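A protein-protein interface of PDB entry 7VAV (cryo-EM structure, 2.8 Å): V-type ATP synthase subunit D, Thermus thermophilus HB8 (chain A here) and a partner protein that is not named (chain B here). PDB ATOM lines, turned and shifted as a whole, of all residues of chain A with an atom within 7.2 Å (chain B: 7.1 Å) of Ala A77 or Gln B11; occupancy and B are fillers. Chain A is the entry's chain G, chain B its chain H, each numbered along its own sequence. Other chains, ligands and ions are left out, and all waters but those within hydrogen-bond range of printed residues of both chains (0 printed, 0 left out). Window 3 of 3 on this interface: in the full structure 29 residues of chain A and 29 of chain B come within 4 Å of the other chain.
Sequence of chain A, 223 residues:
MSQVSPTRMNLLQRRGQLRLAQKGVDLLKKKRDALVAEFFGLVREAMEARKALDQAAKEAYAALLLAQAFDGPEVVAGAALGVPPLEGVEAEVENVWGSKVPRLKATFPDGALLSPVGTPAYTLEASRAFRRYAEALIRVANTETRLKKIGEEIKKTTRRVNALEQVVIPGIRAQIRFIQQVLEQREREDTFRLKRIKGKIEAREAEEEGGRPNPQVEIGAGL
NH2 of Arg B14 sits at hydrogen-bond distance from O of Gly B20 (2.5 Å).
Leu A64 touches Gly B12 (CD1 to CA, 3.7 Å).
Leu B15 touches Val A76 (CD2 to CG2, 3.9 Å).
Ala A77 touches Gln B11 (CA to OE1, 3.99 Å).
Gln B11 touches Ala A80.
O of Arg B14 touches CB of Ala A80 (3.6 Å).
Leu B15 touches Ala A80 (N to CB, 3.5 Å).
Thr A123 touches Leu B15.
Gly B12 touches Phe A130 (O to CE2, 3.1 Å).
CB of Phe A130 touches CB of Ala B16, 3.5 Å away.
Of the printed residues of chain B, Ala A77 touches Gln B11 (3.99 Å).
Gly A78 touches none of the printed residues of chain B.
Printed residues of chain B within 4 Å of Ala A80: Gln B11, Arg B14 and Leu B15.
Gly A82 touches none of the printed residues of chain B.
Printed residues of chain A within 4 Å of Gln B11: Ala A77 (3.99 Å) and Ala A80 (3.9 Å).
Of the printed residues of chain A, Gly B12 touches Leu A64 (3.7 Å) and Phe A130 (3.1 Å).
Of the printed residues of chain A, Arg B14 touches Ala A80 (3.6 Å).
Of the printed residues of chain A, Leu B15 touches Val A76, Ala A80 and Thr A123.
Printed residues of chain A within 4 Å of Ala B16: Phe A130.
The nearest printed residue of chain A that does not touch Leu B15 is Ala A79 (4.1 Å).
Hydrophobic or aromatic side chains of chain A that line the printed part of chain B: Leu A64, Val A76, Ala A80 and Phe A130.
Of the 15 printed residues of chain B, 5 touch a printed residue of chain A.
Among the printed residues, 9 pairs touch across the chains.
Among the printed residues, no Asp or Glu carboxylate lies within 4 Å of a Lys or Arg side-chain nitrogen of the other chain.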
ATOM      1  N   LEU A  64      25.816  -2.870   3.875  1.00  0.00           N
ATOM      2  CA  LEU A  64      24.536  -2.566   4.511  1.00  0.00           C
ATOM      3  C   LEU A  64      24.211  -3.565   5.613  1.00  0.00           C
ATOM      4  O   LEU A  64      23.702  -3.181   6.672  1.00  0.00           O
ATOM      5  CB  LEU A  64      23.410  -2.542   3.470  1.00  0.00           C
ATOM      6  CG  LEU A  64      22.003  -2.130   3.940  1.00  0.00           C
ATOM      7  CD1 LEU A  64      21.225  -1.463   2.824  1.00  0.00           C
ATOM      8  CD2 LEU A  64      21.199  -3.319   4.462  1.00  0.00           C
ATOM      9  N   GLN A  68      22.613  -2.395   9.763  1.00  0.00           N
ATOM     10  CA  GLN A  68      21.329  -2.597  10.422  1.00  0.00           C
ATOM     11  C   GLN A  68      21.375  -3.666  11.505  1.00  0.00           C
ATOM     12  O   GLN A  68      20.425  -3.768  12.290  1.00  0.00           O
ATOM     13  CB  GLN A  68      20.253  -2.945   9.384  1.00  0.00           C
ATOM     14  CG  GLN A  68      20.462  -4.259   8.638  1.00  0.00           C
ATOM     15  CD  GLN A  68      19.905  -5.461   9.382  1.00  0.00           C
ATOM     16  OE1 GLN A  68      18.929  -5.348  10.123  1.00  0.00           O
ATOM     17  NE2 GLN A  68      20.528  -6.617   9.188  1.00  0.00           N
ATOM     18  N   GLY A  72      21.304  -0.167  15.699  1.00  0.00           N
ATOM     19  CA  GLY A  72      19.867  -0.288  15.727  1.00  0.00           C
ATOM     20  C   GLY A  72      19.200   0.361  14.532  1.00  0.00           C
ATOM     21  O   GLY A  72      19.784   1.208  13.848  1.00  0.00           O
ATOM     22  N   PRO A  73      17.956  -0.042  14.249  1.00  0.00           N
ATOM     23  CA  PRO A  73      17.230   0.575  13.125  1.00  0.00           C
ATOM     24  C   PRO A  73      17.049   2.074  13.278  1.00  0.00           C
ATOM     25  O   PRO A  73      17.089   2.806  12.280  1.00  0.00           O
ATOM     26  CB  PRO A  73      15.884  -0.166  13.132  1.00  0.00           C
ATOM     27  CG  PRO A  73      16.146  -1.440  13.872  1.00  0.00           C
ATOM     28  CD  PRO A  73      17.171  -1.098  14.907  1.00  0.00           C
ATOM     29  N   GLU A  74      16.850   2.557  14.506  1.00  0.00           N
ATOM     30  CA  GLU A  74      16.683   3.991  14.712  1.00  0.00           C
ATOM     31  C   GLU A  74      17.971   4.753  14.436  1.00  0.00           C
ATOM     32  O   GLU A  74      17.926   5.881  13.935  1.00  0.00           O
ATOM     33  CB  GLU A  74      16.187   4.262  16.133  1.00  0.00           C
ATOM     34  CG  GLU A  74      14.707   3.969  16.336  1.00  0.00           C
ATOM     35  CD  GLU A  74      14.443   2.547  16.793  1.00  0.00           C
ATOM     36  OE1 GLU A  74      15.256   1.654  16.474  1.00  0.00           O
ATOM     37  OE2 GLU A  74      13.417   2.321  17.469  1.00  0.00           O
ATOM     38  N   VAL A  75      19.126   4.155  14.740  1.00  0.00           N
ATOM     39  CA  VAL A  75      20.400   4.823  14.485  1.00  0.00           C
ATOM     40  C   VAL A  75      20.598   5.044  12.989  1.00  0.00           C
ATOM     41  O   VAL A  75      20.912   6.155  12.539  1.00  0.00           O
ATOM     42  CB  VAL A  75      21.561   4.015  15.092  1.00  0.00           C
ATOM     43  CG1 VAL A  75      22.879   4.750  14.899  1.00  0.00           C
ATOM     44  CG2 VAL A  75      21.302   3.745  16.567  1.00  0.00           C
ATOM     45  N   VAL A  76      20.409   3.989  12.193  1.00  0.00           N
ATOM     46  CA  VAL A  76      20.589   4.115  10.750  1.00  0.00           C
ATOM     47  C   VAL A  76      19.490   4.984  10.148  1.00  0.00           C
ATOM     48  O   VAL A  76      19.719   5.703   9.168  1.00  0.00           O
ATOM     49  CB  VAL A  76      20.658   2.723  10.090  1.00  0.00           C
ATOM     50  CG1 VAL A  76      19.374   1.944  10.312  1.00  0.00           C
ATOM     51  CG2 VAL A  76      20.969   2.847   8.603  1.00  0.00           C
ATOM     52  N   ALA A  77      18.287   4.952  10.729  1.00  0.00           N
ATOM     53  CA  ALA A  77      17.221   5.830  10.254  1.00  0.00           C
ATOM     54  C   ALA A  77      17.571   7.297  10.479  1.00  0.00           C
ATOM     55  O   ALA A  77      17.358   8.138   9.597  1.00  0.00           O
ATOM     56  CB  ALA A  77      15.903   5.478  10.945  1.00  0.00           C
ATOM     57  N   GLY A  78      18.115   7.621  11.654  1.00  0.00           N
ATOM     58  CA  GLY A  78      18.544   8.985  11.907  1.00  0.00           C
ATOM     59  C   GLY A  78      19.706   9.397  11.027  1.00  0.00           C
ATOM     60  O   GLY A  78      19.787  10.547  10.587  1.00  0.00           O
ATOM     61  N   ALA A  79      20.625   8.465  10.761  1.00  0.00           N
ATOM     62  CA  ALA A  79      21.715   8.752   9.832  1.00  0.00           C
ATOM     63  C   ALA A  79      21.182   9.052   8.436  1.00  0.00           C
ATOM     64  O   ALA A  79      21.663   9.971   7.763  1.00  0.00           O
ATOM     65  CB  ALA A  79      22.693   7.578   9.793  1.00  0.00           C
ATOM     66  N   ALA A  80      20.188   8.282   7.985  1.00  0.00           N
ATOM     67  CA  ALA A  80      19.580   8.531   6.682  1.00  0.00           C
ATOM     68  C   ALA A  80      18.871   9.878   6.649  1.00  0.00           C
ATOM     69  O   ALA A  80      18.969  10.614   5.660  1.00  0.00           O
ATOM     70  CB  ALA A  80      18.604   7.406   6.339  1.00  0.00           C
ATOM     71  N   LEU A  81      18.149  10.215   7.719  1.00  0.00           N
ATOM     72  CA  LEU A  81      17.409  11.472   7.745  1.00  0.00           C
ATOM     73  C   LEU A  81      18.336  12.675   7.861  1.00  0.00           C
ATOM     74  O   LEU A  81      17.983  13.772   7.413  1.00  0.00           O
ATOM     75  CB  LEU A  81      16.402  11.463   8.895  1.00  0.00           C
ATOM     76  CG  LEU A  81      15.191  10.546   8.712  1.00  0.00           C
ATOM     77  CD1 LEU A  81      14.466  10.342  10.033  1.00  0.00           C
ATOM     78  CD2 LEU A  81      14.249  11.105   7.657  1.00  0.00           C
ATOM     79  N   GLY A  82      19.515  12.495   8.459  1.00  0.00           N
ATOM     80  CA  GLY A  82      20.413  13.621   8.656  1.00  0.00           C
ATOM     81  C   GLY A  82      20.950  14.197   7.359  1.00  0.00           C
ATOM     82  O   GLY A  82      20.996  15.418   7.185  1.00  0.00           O
ATOM     83  N   VAL A 117      24.430  12.458  11.790  1.00  0.00           N
ATOM     84  CA  VAL A 117      24.613  12.128  13.198  1.00  0.00           C
ATOM     85  C   VAL A 117      24.919  10.651  13.412  1.00  0.00           C
ATOM     86  O   VAL A 117      25.309  10.256  14.518  1.00  0.00           O
ATOM     87  CB  VAL A 117      23.353  12.560  13.982  1.00  0.00           C
ATOM     88  CG1 VAL A 117      22.138  11.747  13.543  1.00  0.00           C
ATOM     89  CG2 VAL A 117      23.572  12.493  15.492  1.00  0.00           C
ATOM     90  N   THR A 123      27.717   2.221   9.850  1.00  0.00           N
ATOM     91  CA  THR A 123      26.838   3.052   9.036  1.00  0.00           C
ATOM     92  C   THR A 123      27.628   3.819   7.980  1.00  0.00           C
ATOM     93  O   THR A 123      27.160   3.986   6.846  1.00  0.00           O
ATOM     94  CB  THR A 123      26.052   4.011   9.934  1.00  0.00           C
ATOM     95  OG1 THR A 123      25.071   3.275  10.675  1.00  0.00           O
ATOM     96  CG2 THR A 123      25.348   5.080   9.111  1.00  0.00           C
ATOM     97  N   PHE A 130      27.447   2.716  -1.216  1.00  0.00           N
ATOM     98  CA  PHE A 130      26.318   3.131  -2.043  1.00  0.00           C
ATOM     99  C   PHE A 130      26.713   4.202  -3.052  1.00  0.00           C
ATOM    100  O   PHE A 130      26.232   4.184  -4.188  1.00  0.00           O
ATOM    101  CB  PHE A 130      25.179   3.625  -1.159  1.00  0.00           C
ATOM    102  CG  PHE A 130      24.456   2.527  -0.445  1.00  0.00           C
ATOM    103  CD1 PHE A 130      24.581   1.216  -0.869  1.00  0.00           C
ATOM    104  CD2 PHE A 130      23.657   2.798   0.651  1.00  0.00           C
ATOM    105  CE1 PHE A 130      23.921   0.198  -0.221  1.00  0.00           C
ATOM    106  CE2 PHE A 130      22.997   1.782   1.305  1.00  0.00           C
ATOM    107  CZ  PHE A 130      23.130   0.482   0.866  1.00  0.00           C
ATOM    108  N   ASP B   6      12.247  -3.009  -2.593  1.00  0.00           N
ATOM    109  CA  ASP B   6      11.691  -3.483  -1.337  1.00  0.00           C
ATOM    110  C   ASP B   6      11.998  -2.487  -0.218  1.00  0.00           C
ATOM    111  O   ASP B   6      12.960  -1.719  -0.309  1.00  0.00           O
ATOM    112  CB  ASP B   6      12.254  -4.862  -0.993  1.00  0.00           C
ATOM    113  CG  ASP B   6      13.769  -4.886  -0.969  1.00  0.00           C
ATOM    114  OD1 ASP B   6      14.359  -4.409   0.023  1.00  0.00           O
ATOM    115  OD2 ASP B   6      14.371  -5.384  -1.943  1.00  0.00           O
ATOM    116  N   PRO B   7      11.183  -2.467   0.843  1.00  0.00           N
ATOM    117  CA  PRO B   7      11.402  -1.477   1.914  1.00  0.00           C
ATOM    118  C   PRO B   7      12.772  -1.566   2.564  1.00  0.00           C
ATOM    119  O   PRO B   7      13.311  -0.534   2.984  1.00  0.00           O
ATOM    120  CB  PRO B   7      10.280  -1.788   2.917  1.00  0.00           C
ATOM    121  CG  PRO B   7       9.809  -3.166   2.570  1.00  0.00           C
ATOM    122  CD  PRO B   7       9.984  -3.284   1.092  1.00  0.00           C
ATOM    123  N   GLU B   8      13.350  -2.765   2.671  1.00  0.00           N
ATOM    124  CA  GLU B   8      14.698  -2.883   3.218  1.00  0.00           C
ATOM    125  C   GLU B   8      15.714  -2.168   2.336  1.00  0.00           C
ATOM    126  O   GLU B   8      16.614  -1.486   2.839  1.00  0.00           O
ATOM    127  CB  GLU B   8      15.069  -4.356   3.390  1.00  0.00           C
ATOM    128  CG  GLU B   8      14.153  -5.119   4.332  1.00  0.00           C
ATOM    129  CD  GLU B   8      13.173  -6.014   3.598  1.00  0.00           C
ATOM    130  OE1 GLU B   8      12.508  -5.526   2.660  1.00  0.00           O
ATOM    131  OE2 GLU B   8      13.069  -7.205   3.958  1.00  0.00           O
ATOM    132  N   THR B   9      15.586  -2.316   1.015  1.00  0.00           N
ATOM    133  CA  THR B   9      16.459  -1.589   0.098  1.00  0.00           C
ATOM    134  C   THR B   9      16.191  -0.090   0.159  1.00  0.00           C
ATOM    135  O   THR B   9      17.118   0.721   0.031  1.00  0.00           O
ATOM    136  CB  THR B   9      16.269  -2.111  -1.327  1.00  0.00           C
ATOM    137  OG1 THR B   9      16.444  -3.532  -1.344  1.00  0.00           O
ATOM    138  CG2 THR B   9      17.286  -1.488  -2.261  1.00  0.00           C
ATOM    139  N   ALA B  10      14.926   0.293   0.351  1.00  0.00           N
ATOM    140  CA  ALA B  10      14.576   1.707   0.424  1.00  0.00           C
ATOM    141  C   ALA B  10      15.273   2.390   1.594  1.00  0.00           C
ATOM    142  O   ALA B  10      15.686   3.549   1.485  1.00  0.00           O
ATOM    143  CB  ALA B  10      13.060   1.869   0.531  1.00  0.00           C
ATOM    144  N   GLN B  11      15.407   1.689   2.722  1.00  0.00           N
ATOM    145  CA  GLN B  11      16.133   2.253   3.856  1.00  0.00           C
ATOM    146  C   GLN B  11      17.583   2.542   3.489  1.00  0.00           C
ATOM    147  O   GLN B  11      18.118   3.607   3.820  1.00  0.00           O
ATOM    148  CB  GLN B  11      16.060   1.302   5.051  1.00  0.00           C
ATOM    149  CG  GLN B  11      16.657   1.861   6.333  1.00  0.00           C
ATOM    150  CD  GLN B  11      15.897   3.064   6.856  1.00  0.00           C
ATOM    151  OE1 GLN B  11      16.343   4.203   6.720  1.00  0.00           O
ATOM    152  NE2 GLN B  11      14.741   2.815   7.462  1.00  0.00           N
ATOM    153  N   GLY B  12      18.231   1.612   2.784  1.00  0.00           N
ATOM    154  CA  GLY B  12      19.600   1.847   2.355  1.00  0.00           C
ATOM    155  C   GLY B  12      19.717   3.001   1.376  1.00  0.00           C
ATOM    156  O   GLY B  12      20.661   3.790   1.443  1.00  0.00           O
ATOM    157  N   PHE B  13      18.761   3.114   0.452  1.00  0.00           N
ATOM    158  CA  PHE B  13      18.809   4.210  -0.511  1.00  0.00           C
ATOM    159  C   PHE B  13      18.575   5.557   0.163  1.00  0.00           C
ATOM    160  O   PHE B  13      19.181   6.564  -0.224  1.00  0.00           O
ATOM    161  CB  PHE B  13      17.804   3.969  -1.637  1.00  0.00           C
ATOM    162  CG  PHE B  13      18.369   3.173  -2.778  1.00  0.00           C
ATOM    163  CD1 PHE B  13      19.424   3.671  -3.525  1.00  0.00           C
ATOM    164  CD2 PHE B  13      17.869   1.921  -3.088  1.00  0.00           C
ATOM    165  CE1 PHE B  13      19.958   2.945  -4.572  1.00  0.00           C
ATOM    166  CE2 PHE B  13      18.404   1.188  -4.133  1.00  0.00           C
ATOM    167  CZ  PHE B  13      19.447   1.702  -4.875  1.00  0.00           C
ATOM    168  N   ARG B  14      17.700   5.600   1.172  1.00  0.00           N
ATOM    169  CA  ARG B  14      17.569   6.815   1.973  1.00  0.00           C
ATOM    170  C   ARG B  14      18.859   7.110   2.727  1.00  0.00           C
ATOM    171  O   ARG B  14      19.235   8.276   2.897  1.00  0.00           O
ATOM    172  CB  ARG B  14      16.394   6.692   2.944  1.00  0.00           C
ATOM    173  CG  ARG B  14      15.045   6.488   2.277  1.00  0.00           C
ATOM    174  CD  ARG B  14      14.498   7.794   1.724  1.00  0.00           C
ATOM    175  NE  ARG B  14      13.347   7.577   0.856  1.00  0.00           N
ATOM    176  CZ  ARG B  14      12.517   8.532   0.460  1.00  0.00           C
ATOM    177  NH1 ARG B  14      12.683   9.790   0.830  1.00  0.00           N
ATOM    178  NH2 ARG B  14      11.491   8.214  -0.325  1.00  0.00           N
ATOM    179  N   LEU B  15      19.546   6.065   3.197  1.00  0.00           N
ATOM    180  CA  LEU B  15      20.855   6.254   3.814  1.00  0.00           C
ATOM    181  C   LEU B  15      21.852   6.846   2.828  1.00  0.00           C
ATOM    182  O   LEU B  15      22.713   7.645   3.216  1.00  0.00           O
ATOM    183  CB  LEU B  15      21.371   4.923   4.364  1.00  0.00           C
ATOM    184  CG  LEU B  15      22.798   4.890   4.915  1.00  0.00           C
ATOM    185  CD1 LEU B  15      22.984   5.934   6.008  1.00  0.00           C
ATOM    186  CD2 LEU B  15      23.145   3.501   5.428  1.00  0.00           C
ATOM    187  N   ALA B  16      21.746   6.479   1.555  1.00  0.00           N
ATOM    188  CA  ALA B  16      22.628   6.982   0.512  1.00  0.00           C
ATOM    189  C   ALA B  16      22.250   8.376   0.034  1.00  0.00           C
ATOM    190  O   ALA B  16      22.977   8.954  -0.781  1.00  0.00           O
ATOM    191  CB  ALA B  16      22.633   6.021  -0.681  1.00  0.00           C
ATOM    192  N   GLY B  17      21.139   8.930   0.516  1.00  0.00           N
ATOM    193  CA  GLY B  17      20.646  10.202   0.042  1.00  0.00           C
ATOM    194  C   GLY B  17      19.675  10.116  -1.114  1.00  0.00           C
ATOM    195  O   GLY B  17      19.157  11.153  -1.547  1.00  0.00           O
ATOM    196  N   LEU B  18      19.411   8.918  -1.627  1.00  0.00           N
ATOM    197  CA  LEU B  18      18.458   8.748  -2.712  1.00  0.00           C
ATOM    198  C   LEU B  18      17.050   8.562  -2.158  1.00  0.00           C
ATOM    199  O   LEU B  18      16.856   8.053  -1.052  1.00  0.00           O
ATOM    200  CB  LEU B  18      18.842   7.552  -3.586  1.00  0.00           C
ATOM    201  CG  LEU B  18      19.915   7.798  -4.651  1.00  0.00           C
ATOM    202  CD1 LEU B  18      21.312   7.782  -4.045  1.00  0.00           C
ATOM    203  CD2 LEU B  18      19.805   6.778  -5.773  1.00  0.00           C
ATOM    204  N   GLY B  20      14.562   6.629  -1.875  1.00  0.00           N
ATOM    205  CA  GLY B  20      14.125   5.251  -1.977  1.00  0.00           C
ATOM    206  C   GLY B  20      12.651   5.089  -1.656  1.00  0.00           C
ATOM    207  O   GLY B  20      12.077   5.825  -0.853  1.00  0.00           O
ATOM    208  N   TYR B  21      12.032   4.103  -2.299  1.00  0.00           N
ATOM    209  CA  TYR B  21      10.614   3.821  -2.122  1.00  0.00           C
ATOM    210  C   TYR B  21      10.409   2.327  -1.931  1.00  0.00           C
ATOM    211  O   TYR B  21      11.143   1.512  -2.500  1.00  0.00           O
ATOM    212  CB  TYR B  21       9.794   4.311  -3.321  1.00  0.00           C
ATOM    213  CG  TYR B  21       9.556   5.803  -3.332  1.00  0.00           C
ATOM    214  CD1 TYR B  21       8.623   6.383  -2.481  1.00  0.00           C
ATOM    215  CD2 TYR B  21      10.262   6.632  -4.192  1.00  0.00           C
ATOM    216  CE1 TYR B  21       8.402   7.747  -2.488  1.00  0.00           C
ATOM    217  CE2 TYR B  21      10.048   7.997  -4.206  1.00  0.00           C
ATOM    218  CZ  TYR B  21       9.117   8.548  -3.351  1.00  0.00           C
ATOM    219  OH  TYR B  21       8.900   9.906  -3.361  1.00  0.00           O
